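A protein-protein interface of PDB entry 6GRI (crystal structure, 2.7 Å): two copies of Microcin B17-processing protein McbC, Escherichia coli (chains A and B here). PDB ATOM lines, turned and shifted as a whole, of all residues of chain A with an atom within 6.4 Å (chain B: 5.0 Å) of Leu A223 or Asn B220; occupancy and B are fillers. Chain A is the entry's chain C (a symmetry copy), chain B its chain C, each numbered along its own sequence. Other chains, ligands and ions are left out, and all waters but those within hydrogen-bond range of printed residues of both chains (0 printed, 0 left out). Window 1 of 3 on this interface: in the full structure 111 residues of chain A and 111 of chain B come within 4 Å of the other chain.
The side-chain amide nitrogen of Gln B219 is in hydrogen-bond range of the side-chain amide oxygen of Asn A220 (2.7 Å).
The backbone carbonyl oxygen (O) of Pro B119 sits at hydrogen-bond distance from the side-chain amide nitrogen (NE2) of Gln A219 (2.8 Å).
The backbone carbonyl oxygen (O) of Tyr B120 lies within hydrogen-bond range of the guanidinium group (NH2) of Arg A82 (3.3 Å).
The side-chain amide nitrogen (NE2) of Gln A219 lies within hydrogen-bond range of the side-chain amide oxygen (OD1) of Asn B220.
O of Pro B119 is in hydrogen-bond range of ND2 of Asn B220 (2.9 Å).
The backbone carbonyl oxygen of Leu A223 is in hydrogen-bond range of the side-chain amide nitrogen of Gln A227 (2.9 Å).
ND2 of Asn B220 sits at hydrogen-bond distance from O of Ala B107 (3.0 Å).
The side-chain sulfur (SD) of Met B217 sits close to the side-chain hydroxyl (OH) of Tyr B120, at 3.5 Å.
Leu A223 touches two residues of chain B.
Asn B220 touches just these residues of chain A: Gln A219 and Leu A223.
Of the printed residues of chain A, Pro B119 touches Arg A82 and Gln A219.
Of the printed residues of chain B, Arg A82 touches Pro B119 (3.6 Å) and Tyr B120 (3.3 Å).
Of the printed residues of chain B, Asn A220 touches Gln B219 and Leu B223.
Of the printed residues of chain B, Gln A219 touches Pro B119 (2.8 Å), Tyr B120 (3.7 Å), Ser B216 (3.6 Å) and Asn B220 (2.7 Å).
Val B222 touches none of the printed residues of chain A.
Met B217 touches none of the printed residues of chain A.
The nearest printed residue of chain A that does not touch Pro B119 is Leu A223 (4.7 Å).
Gln A219 touches Asn B220, and with the chains exchanged Asn A220 touches Gln B219.
Asn A220 touches Leu B223, and with the chains exchanged Leu A223 touches Asn B220.
Leu B223 touches its own counterpart, Leu A223.
Positions printed for both chains: 218, 219, 220, 221, 222, 223, 224 and 225.
Of the 10 pairs that touch across the chains among the printed residues, 5 have their exchanged pair printed and touching as well.
Of the 14 printed residues of chain B, 6 touch a printed residue of chain A.
Of the 13 printed residues of chain A, 4 touch a printed residue of chain B.
Printed residues of chain A that touch a printed residue of chain B: Arg A82, Gln A219, Asn A220 and Leu A223.
Hydrophobic or aromatic side chains of chain A that line the printed part of chain B: Leu A223.
NE of Arg A82 touches C of Pro B119 (3.6 Å).
Gln A219 touches Tyr B120 (OE1 to CB, 3.7 Å).
Gln A219 touches Ser B216.
Asn A220 touches Leu B223.
Asn B220 touches Leu A223 (OD1 to CD1, 3.7 Å).
Leu B223 touches Leu A223 (CD1 to CD1, 3.2 Å).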
ATOM      1  N   ARG A  82      20.791  26.600  21.717  1.00  0.00           N
ATOM      2  CA  ARG A  82      20.684  27.456  22.902  1.00  0.00           C
ATOM      3  C   ARG A  82      19.259  27.966  22.929  1.00  0.00           C
ATOM      4  O   ARG A  82      18.736  28.377  21.888  1.00  0.00           O
ATOM      5  CB  ARG A  82      21.665  28.630  22.798  1.00  0.00           C
ATOM      6  CG  ARG A  82      21.631  29.637  23.946  1.00  0.00           C
ATOM      7  CD  ARG A  82      22.679  30.723  23.754  1.00  0.00           C
ATOM      8  NE  ARG A  82      22.474  31.460  22.505  1.00  0.00           N
ATOM      9  CZ  ARG A  82      21.697  32.537  22.343  1.00  0.00           C
ATOM     10  NH1 ARG A  82      21.017  33.076  23.358  1.00  0.00           N
ATOM     11  NH2 ARG A  82      21.600  33.093  21.136  1.00  0.00           N
ATOM     12  N   TYR A 218      29.669  34.767  31.667  1.00  0.00           N
ATOM     13  CA  TYR A 218      28.219  34.779  31.414  1.00  0.00           C
ATOM     14  C   TYR A 218      27.780  33.716  30.429  1.00  0.00           C
ATOM     15  O   TYR A 218      26.619  33.317  30.454  1.00  0.00           O
ATOM     16  CB  TYR A 218      27.651  36.181  31.061  1.00  0.00           C
ATOM     17  CG  TYR A 218      27.898  36.788  29.679  1.00  0.00           C
ATOM     18  CD1 TYR A 218      27.563  36.104  28.497  1.00  0.00           C
ATOM     19  CD2 TYR A 218      28.369  38.100  29.557  1.00  0.00           C
ATOM     20  CE1 TYR A 218      27.755  36.682  27.253  1.00  0.00           C
ATOM     21  CE2 TYR A 218      28.564  38.683  28.308  1.00  0.00           C
ATOM     22  CZ  TYR A 218      28.256  37.965  27.161  1.00  0.00           C
ATOM     23  OH  TYR A 218      28.442  38.510  25.910  1.00  0.00           O
ATOM     24  N   GLN A 219      28.692  33.262  29.566  1.00  0.00           N
ATOM     25  CA  GLN A 219      28.383  32.188  28.613  1.00  0.00           C
ATOM     26  C   GLN A 219      28.327  30.840  29.318  1.00  0.00           C
ATOM     27  O   GLN A 219      27.410  30.054  29.059  1.00  0.00           O
ATOM     28  CB  GLN A 219      29.386  32.161  27.448  1.00  0.00           C
ATOM     29  CG  GLN A 219      29.164  31.098  26.373  1.00  0.00           C
ATOM     30  CD  GLN A 219      27.837  31.202  25.630  1.00  0.00           C
ATOM     31  OE1 GLN A 219      27.119  32.199  25.719  1.00  0.00           O
ATOM     32  NE2 GLN A 219      27.509  30.150  24.884  1.00  0.00           N
ATOM     33  N   ASN A 220      29.292  30.563  30.201  1.00  0.00           N
ATOM     34  CA  ASN A 220      29.181  29.405  31.113  1.00  0.00           C
ATOM     35  C   ASN A 220      27.851  29.462  31.851  1.00  0.00           C
ATOM     36  O   ASN A 220      27.176  28.451  31.944  1.00  0.00           O
ATOM     37  CB  ASN A 220      30.328  29.339  32.128  1.00  0.00           C
ATOM     38  CG  ASN A 220      31.591  28.705  31.566  1.00  0.00           C
ATOM     39  OD1 ASN A 220      31.748  28.532  30.354  1.00  0.00           O
ATOM     40  ND2 ASN A 220      32.511  28.358  32.466  1.00  0.00           N
ATOM     41  N   ALA A 221      27.459  30.642  32.340  1.00  0.00           N
ATOM     42  CA  ALA A 221      26.138  30.809  32.960  1.00  0.00           C
ATOM     43  C   ALA A 221      25.000  30.484  31.999  1.00  0.00           C
ATOM     44  O   ALA A 221      24.078  29.752  32.369  1.00  0.00           O
ATOM     45  CB  ALA A 221      25.961  32.208  33.525  1.00  0.00           C
ATOM     46  N   VAL A 222      25.074  31.030  30.779  1.00  0.00           N
ATOM     47  CA  VAL A 222      24.104  30.747  29.700  1.00  0.00           C
ATOM     48  C   VAL A 222      23.967  29.248  29.499  1.00  0.00           C
ATOM     49  O   VAL A 222      22.866  28.711  29.581  1.00  0.00           O
ATOM     50  CB  VAL A 222      24.494  31.435  28.358  1.00  0.00           C
ATOM     51  CG1 VAL A 222      23.859  30.758  27.150  1.00  0.00           C
ATOM     52  CG2 VAL A 222      24.109  32.910  28.381  1.00  0.00           C
ATOM     53  N   LEU A 223      25.092  28.580  29.266  1.00  0.00           N
ATOM     54  CA  LEU A 223      25.089  27.131  29.038  1.00  0.00           C
ATOM     55  C   LEU A 223      24.608  26.330  30.257  1.00  0.00           C
ATOM     56  O   LEU A 223      23.813  25.399  30.105  1.00  0.00           O
ATOM     57  CB  LEU A 223      26.473  26.653  28.613  1.00  0.00           C
ATOM     58  CG  LEU A 223      27.023  27.245  27.312  1.00  0.00           C
ATOM     59  CD1 LEU A 223      28.480  26.849  27.137  1.00  0.00           C
ATOM     60  CD2 LEU A 223      26.203  26.806  26.114  1.00  0.00           C
ATOM     61  N   VAL A 224      25.083  26.699  31.451  1.00  0.00           N
ATOM     62  CA  VAL A 224      24.696  26.024  32.710  1.00  0.00           C
ATOM     63  C   VAL A 224      23.192  26.159  32.980  1.00  0.00           C
ATOM     64  O   VAL A 224      22.525  25.158  33.238  1.00  0.00           O
ATOM     65  CB  VAL A 224      25.533  26.531  33.913  1.00  0.00           C
ATOM     66  CG1 VAL A 224      24.916  26.140  35.252  1.00  0.00           C
ATOM     67  CG2 VAL A 224      26.953  25.988  33.822  1.00  0.00           C
ATOM     68  N   ALA A 225      22.680  27.390  32.896  1.00  0.00           N
ATOM     69  CA  ALA A 225      21.246  27.686  33.087  1.00  0.00           C
ATOM     70  C   ALA A 225      20.325  26.848  32.204  1.00  0.00           C
ATOM     71  O   ALA A 225      19.340  26.286  32.689  1.00  0.00           O
ATOM     72  CB  ALA A 225      20.984  29.159  32.839  1.00  0.00           C
ATOM     73  N   ASP A 226      20.650  26.767  30.912  1.00  0.00           N
ATOM     74  CA  ASP A 226      19.898  25.926  29.953  1.00  0.00           C
ATOM     75  C   ASP A 226      19.701  24.491  30.453  1.00  0.00           C
ATOM     76  O   ASP A 226      18.590  23.958  30.408  1.00  0.00           O
ATOM     77  CB  ASP A 226      20.587  25.901  28.577  1.00  0.00           C
ATOM     78  CG  ASP A 226      20.186  27.082  27.688  1.00  0.00           C
ATOM     79  OD1 ASP A 226      20.453  28.254  28.041  1.00  0.00           O
ATOM     80  OD2 ASP A 226      19.610  26.837  26.613  1.00  0.00           O
ATOM     81  N   GLN A 227      20.783  23.898  30.957  1.00  0.00           N
ATOM     82  CA  GLN A 227      20.797  22.500  31.401  1.00  0.00           C
ATOM     83  C   GLN A 227      20.000  22.238  32.667  1.00  0.00           C
ATOM     84  O   GLN A 227      19.609  21.106  32.903  1.00  0.00           O
ATOM     85  CB  GLN A 227      22.230  22.030  31.655  1.00  0.00           C
ATOM     86  CG  GLN A 227      23.124  22.026  30.427  1.00  0.00           C
ATOM     87  CD  GLN A 227      24.592  21.990  30.793  1.00  0.00           C
ATOM     88  OE1 GLN A 227      25.030  21.112  31.538  1.00  0.00           O
ATOM     89  NE2 GLN A 227      25.360  22.938  30.268  1.00  0.00           N
ATOM     90  N   ILE A 228      19.786  23.250  33.500  1.00  0.00           N
ATOM     91  CA  ILE A 228      19.051  23.051  34.757  1.00  0.00           C
ATOM     92  C   ILE A 228      17.644  23.657  34.724  1.00  0.00           C
ATOM     93  O   ILE A 228      16.957  23.667  35.736  1.00  0.00           O
ATOM     94  CB  ILE A 228      19.876  23.527  35.988  1.00  0.00           C
ATOM     95  CG1 ILE A 228      19.846  25.055  36.149  1.00  0.00           C
ATOM     96  CG2 ILE A 228      21.306  22.995  35.892  1.00  0.00           C
ATOM     97  CD1 ILE A 228      20.821  25.600  37.176  1.00  0.00           C
ATOM     98  N   ASN A 232      17.221  32.699  30.778  1.00  0.00           N
ATOM     99  CA  ASN A 232      18.090  33.809  31.190  1.00  0.00           C
ATOM    100  C   ASN A 232      18.144  34.907  30.142  1.00  0.00           C
ATOM    101  O   ASN A 232      17.654  34.753  29.032  1.00  0.00           O
ATOM    102  CB  ASN A 232      19.508  33.296  31.508  1.00  0.00           C
ATOM    103  CG  ASN A 232      20.355  33.054  30.265  1.00  0.00           C
ATOM    104  OD1 ASN A 232      20.935  33.978  29.704  1.00  0.00           O
ATOM    105  ND2 ASN A 232      20.455  31.803  29.855  1.00  0.00           N
ATOM    106  N   ALA B 107      30.737  25.233  18.227  1.00  0.00           N
ATOM    107  CA  ALA B 107      31.022  26.453  19.000  1.00  0.00           C
ATOM    108  C   ALA B 107      30.278  27.717  18.560  1.00  0.00           C
ATOM    109  O   ALA B 107      30.043  28.590  19.407  1.00  0.00           O
ATOM    110  CB  ALA B 107      32.519  26.739  19.015  1.00  0.00           C
ATOM    111  N   PRO B 119      24.780  29.746  19.072  1.00  0.00           N
ATOM    112  CA  PRO B 119      24.902  29.219  20.434  1.00  0.00           C
ATOM    113  C   PRO B 119      25.607  30.158  21.453  1.00  0.00           C
ATOM    114  O   PRO B 119      26.162  29.692  22.443  1.00  0.00           O
ATOM    115  CB  PRO B 119      25.707  27.936  20.216  1.00  0.00           C
ATOM    116  CG  PRO B 119      26.598  28.253  19.076  1.00  0.00           C
ATOM    117  CD  PRO B 119      25.918  29.305  18.246  1.00  0.00           C
ATOM    118  N   TYR B 120      25.601  31.459  21.189  1.00  0.00           N
ATOM    119  CA  TYR B 120      25.994  32.468  22.162  1.00  0.00           C
ATOM    120  C   TYR B 120      25.168  33.716  21.865  1.00  0.00           C
ATOM    121  O   TYR B 120      24.744  33.917  20.722  1.00  0.00           O
ATOM    122  CB  TYR B 120      27.500  32.758  22.092  1.00  0.00           C
ATOM    123  CG  TYR B 120      27.991  33.260  20.740  1.00  0.00           C
ATOM    124  CD1 TYR B 120      28.222  32.377  19.683  1.00  0.00           C
ATOM    125  CD2 TYR B 120      28.238  34.617  20.523  1.00  0.00           C
ATOM    126  CE1 TYR B 120      28.673  32.830  18.448  1.00  0.00           C
ATOM    127  CE2 TYR B 120      28.687  35.076  19.295  1.00  0.00           C
ATOM    128  CZ  TYR B 120      28.898  34.181  18.258  1.00  0.00           C
ATOM    129  OH  TYR B 120      29.344  34.633  17.038  1.00  0.00           O
ATOM    130  N   GLY B 215      34.668  36.751  24.293  1.00  0.00           N
ATOM    131  CA  GLY B 215      34.955  35.764  25.309  1.00  0.00           C
ATOM    132  C   GLY B 215      33.939  34.654  25.345  1.00  0.00           C
ATOM    133  O   GLY B 215      34.314  33.493  25.565  1.00  0.00           O
ATOM    134  N   SER B 216      32.659  34.996  25.135  1.00  0.00           N
ATOM    135  CA  SER B 216      31.602  33.974  25.010  1.00  0.00           C
ATOM    136  C   SER B 216      31.961  33.007  23.890  1.00  0.00           C
ATOM    137  O   SER B 216      31.782  31.796  24.016  1.00  0.00           O
ATOM    138  CB  SER B 216      30.211  34.593  24.772  1.00  0.00           C
ATOM    139  OG  SER B 216      30.035  35.098  23.458  1.00  0.00           O
ATOM    140  N   MET B 217      32.515  33.551  22.810  1.00  0.00           N
ATOM    141  CA  MET B 217      32.900  32.742  21.654  1.00  0.00           C
ATOM    142  C   MET B 217      34.059  31.794  21.942  1.00  0.00           C
ATOM    143  O   MET B 217      33.907  30.577  21.750  1.00  0.00           O
ATOM    144  CB  MET B 217      33.165  33.638  20.449  1.00  0.00           C
ATOM    145  CG  MET B 217      31.869  34.253  19.951  1.00  0.00           C
ATOM    146  SD  MET B 217      32.096  35.653  18.866  1.00  0.00           S
ATOM    147  CE  MET B 217      32.603  34.800  17.375  1.00  0.00           C
ATOM    148  N   TYR B 218      35.180  32.329  22.441  1.00  0.00           N
ATOM    149  CA  TYR B 218      36.346  31.484  22.744  1.00  0.00           C
ATOM    150  C   TYR B 218      36.084  30.488  23.855  1.00  0.00           C
ATOM    151  O   TYR B 218      36.762  29.466  23.916  1.00  0.00           O
ATOM    152  CB  TYR B 218      37.663  32.279  22.964  1.00  0.00           C
ATOM    153  CG  TYR B 218      37.887  33.057  24.261  1.00  0.00           C
ATOM    154  CD1 TYR B 218      37.781  32.443  25.523  1.00  0.00           C
ATOM    155  CD2 TYR B 218      38.317  34.388  24.223  1.00  0.00           C
ATOM    156  CE1 TYR B 218      38.026  33.149  26.688  1.00  0.00           C
ATOM    157  CE2 TYR B 218      38.563  35.100  25.392  1.00  0.00           C
ATOM    158  CZ  TYR B 218      38.412  34.474  26.622  1.00  0.00           C
ATOM    159  OH  TYR B 218      38.642  35.151  27.798  1.00  0.00           O
ATOM    160  N   GLN B 219      35.117  30.780  24.728  1.00  0.00           N
ATOM    161  CA  GLN B 219      34.744  29.851  25.803  1.00  0.00           C
ATOM    162  C   GLN B 219      33.942  28.681  25.251  1.00  0.00           C
ATOM    163  O   GLN B 219      34.201  27.533  25.628  1.00  0.00           O
ATOM    164  CB  GLN B 219      33.976  30.567  26.926  1.00  0.00           C
ATOM    165  CG  GLN B 219      33.544  29.712  28.117  1.00  0.00           C
ATOM    166  CD  GLN B 219      34.687  29.067  28.894  1.00  0.00           C
ATOM    167  OE1 GLN B 219      35.860  29.405  28.723  1.00  0.00           O
ATOM    168  NE2 GLN B 219      34.335  28.123  29.761  1.00  0.00           N
ATOM    169  N   ASN B 220      32.976  28.954  24.368  1.00  0.00           N
ATOM    170  CA  ASN B 220      32.326  27.876  23.592  1.00  0.00           C
ATOM    171  C   ASN B 220      33.388  27.032  22.902  1.00  0.00           C
ATOM    172  O   ASN B 220      33.304  25.817  22.945  1.00  0.00           O
ATOM    173  CB  ASN B 220      31.339  28.412  22.548  1.00  0.00           C
ATOM    174  CG  ASN B 220      29.973  28.742  23.129  1.00  0.00           C
ATOM    175  OD1 ASN B 220      29.788  28.834  24.346  1.00  0.00           O
ATOM    176  ND2 ASN B 220      28.999  28.932  22.238  1.00  0.00           N
ATOM    177  N   ALA B 221      34.398  27.669  22.302  1.00  0.00           N
ATOM    178  CA  ALA B 221      35.524  26.929  21.717  1.00  0.00           C
ATOM    179  C   ALA B 221      36.264  26.085  22.750  1.00  0.00           C
ATOM    180  O   ALA B 221      36.536  24.909  22.496  1.00  0.00           O
ATOM    181  CB  ALA B 221      36.495  27.859  21.010  1.00  0.00           C
ATOM    182  N   VAL B 222      36.583  26.692  23.899  1.00  0.00           N
ATOM    183  CA  VAL B 222      37.220  25.997  25.038  1.00  0.00           C
ATOM    184  C   VAL B 222      36.424  24.757  25.406  1.00  0.00           C
ATOM    185  O   VAL B 222      36.967  23.656  25.423  1.00  0.00           O
ATOM    186  CB  VAL B 222      37.379  26.921  26.282  1.00  0.00           C
ATOM    187  CG1 VAL B 222      37.515  26.133  27.579  1.00  0.00           C
ATOM    188  CG2 VAL B 222      38.580  27.843  26.113  1.00  0.00           C
ATOM    189  N   LEU B 223      35.134  24.941  25.668  1.00  0.00           N
ATOM    190  CA  LEU B 223      34.264  23.825  26.051  1.00  0.00           C
ATOM    191  C   LEU B 223      34.113  22.770  24.946  1.00  0.00           C
ATOM    192  O   LEU B 223      34.183  21.571  25.228  1.00  0.00           O
ATOM    193  CB  LEU B 223      32.891  24.337  26.475  1.00  0.00           C
ATOM    194  CG  LEU B 223      32.864  25.279  27.682  1.00  0.00           C
ATOM    195  CD1 LEU B 223      31.474  25.873  27.845  1.00  0.00           C
ATOM    196  CD2 LEU B 223      33.291  24.565  28.951  1.00  0.00           C
ATOM    197  N   VAL B 224      33.916  23.220  23.702  1.00  0.00           N
ATOM    198  CA  VAL B 224      33.767  22.316  22.539  1.00  0.00           C
ATOM    199  C   VAL B 224      35.030  21.479  22.312  1.00  0.00           C
ATOM    200  O   VAL B 224      34.941  20.257  22.189  1.00  0.00           O
ATOM    201  CB  VAL B 224      33.367  23.093  21.258  1.00  0.00           C
ATOM    202  CG1 VAL B 224      33.568  22.265  19.993  1.00  0.00           C
ATOM    203  CG2 VAL B 224      31.914  23.540  21.354  1.00  0.00           C
ATOM    204  N   ALA B 225      36.188  22.144  22.280  1.00  0.00           N
ATOM    205  CA  ALA B 225      37.498  21.484  22.112  1.00  0.00           C
ATOM    206  C   ALA B 225      37.751  20.361  23.114  1.00  0.00           C
ATOM    207  O   ALA B 225      38.172  19.267  22.730  1.00  0.00           O
ATOM    208  CB  ALA B 225      38.612  22.510  22.208  1.00  0.00           C
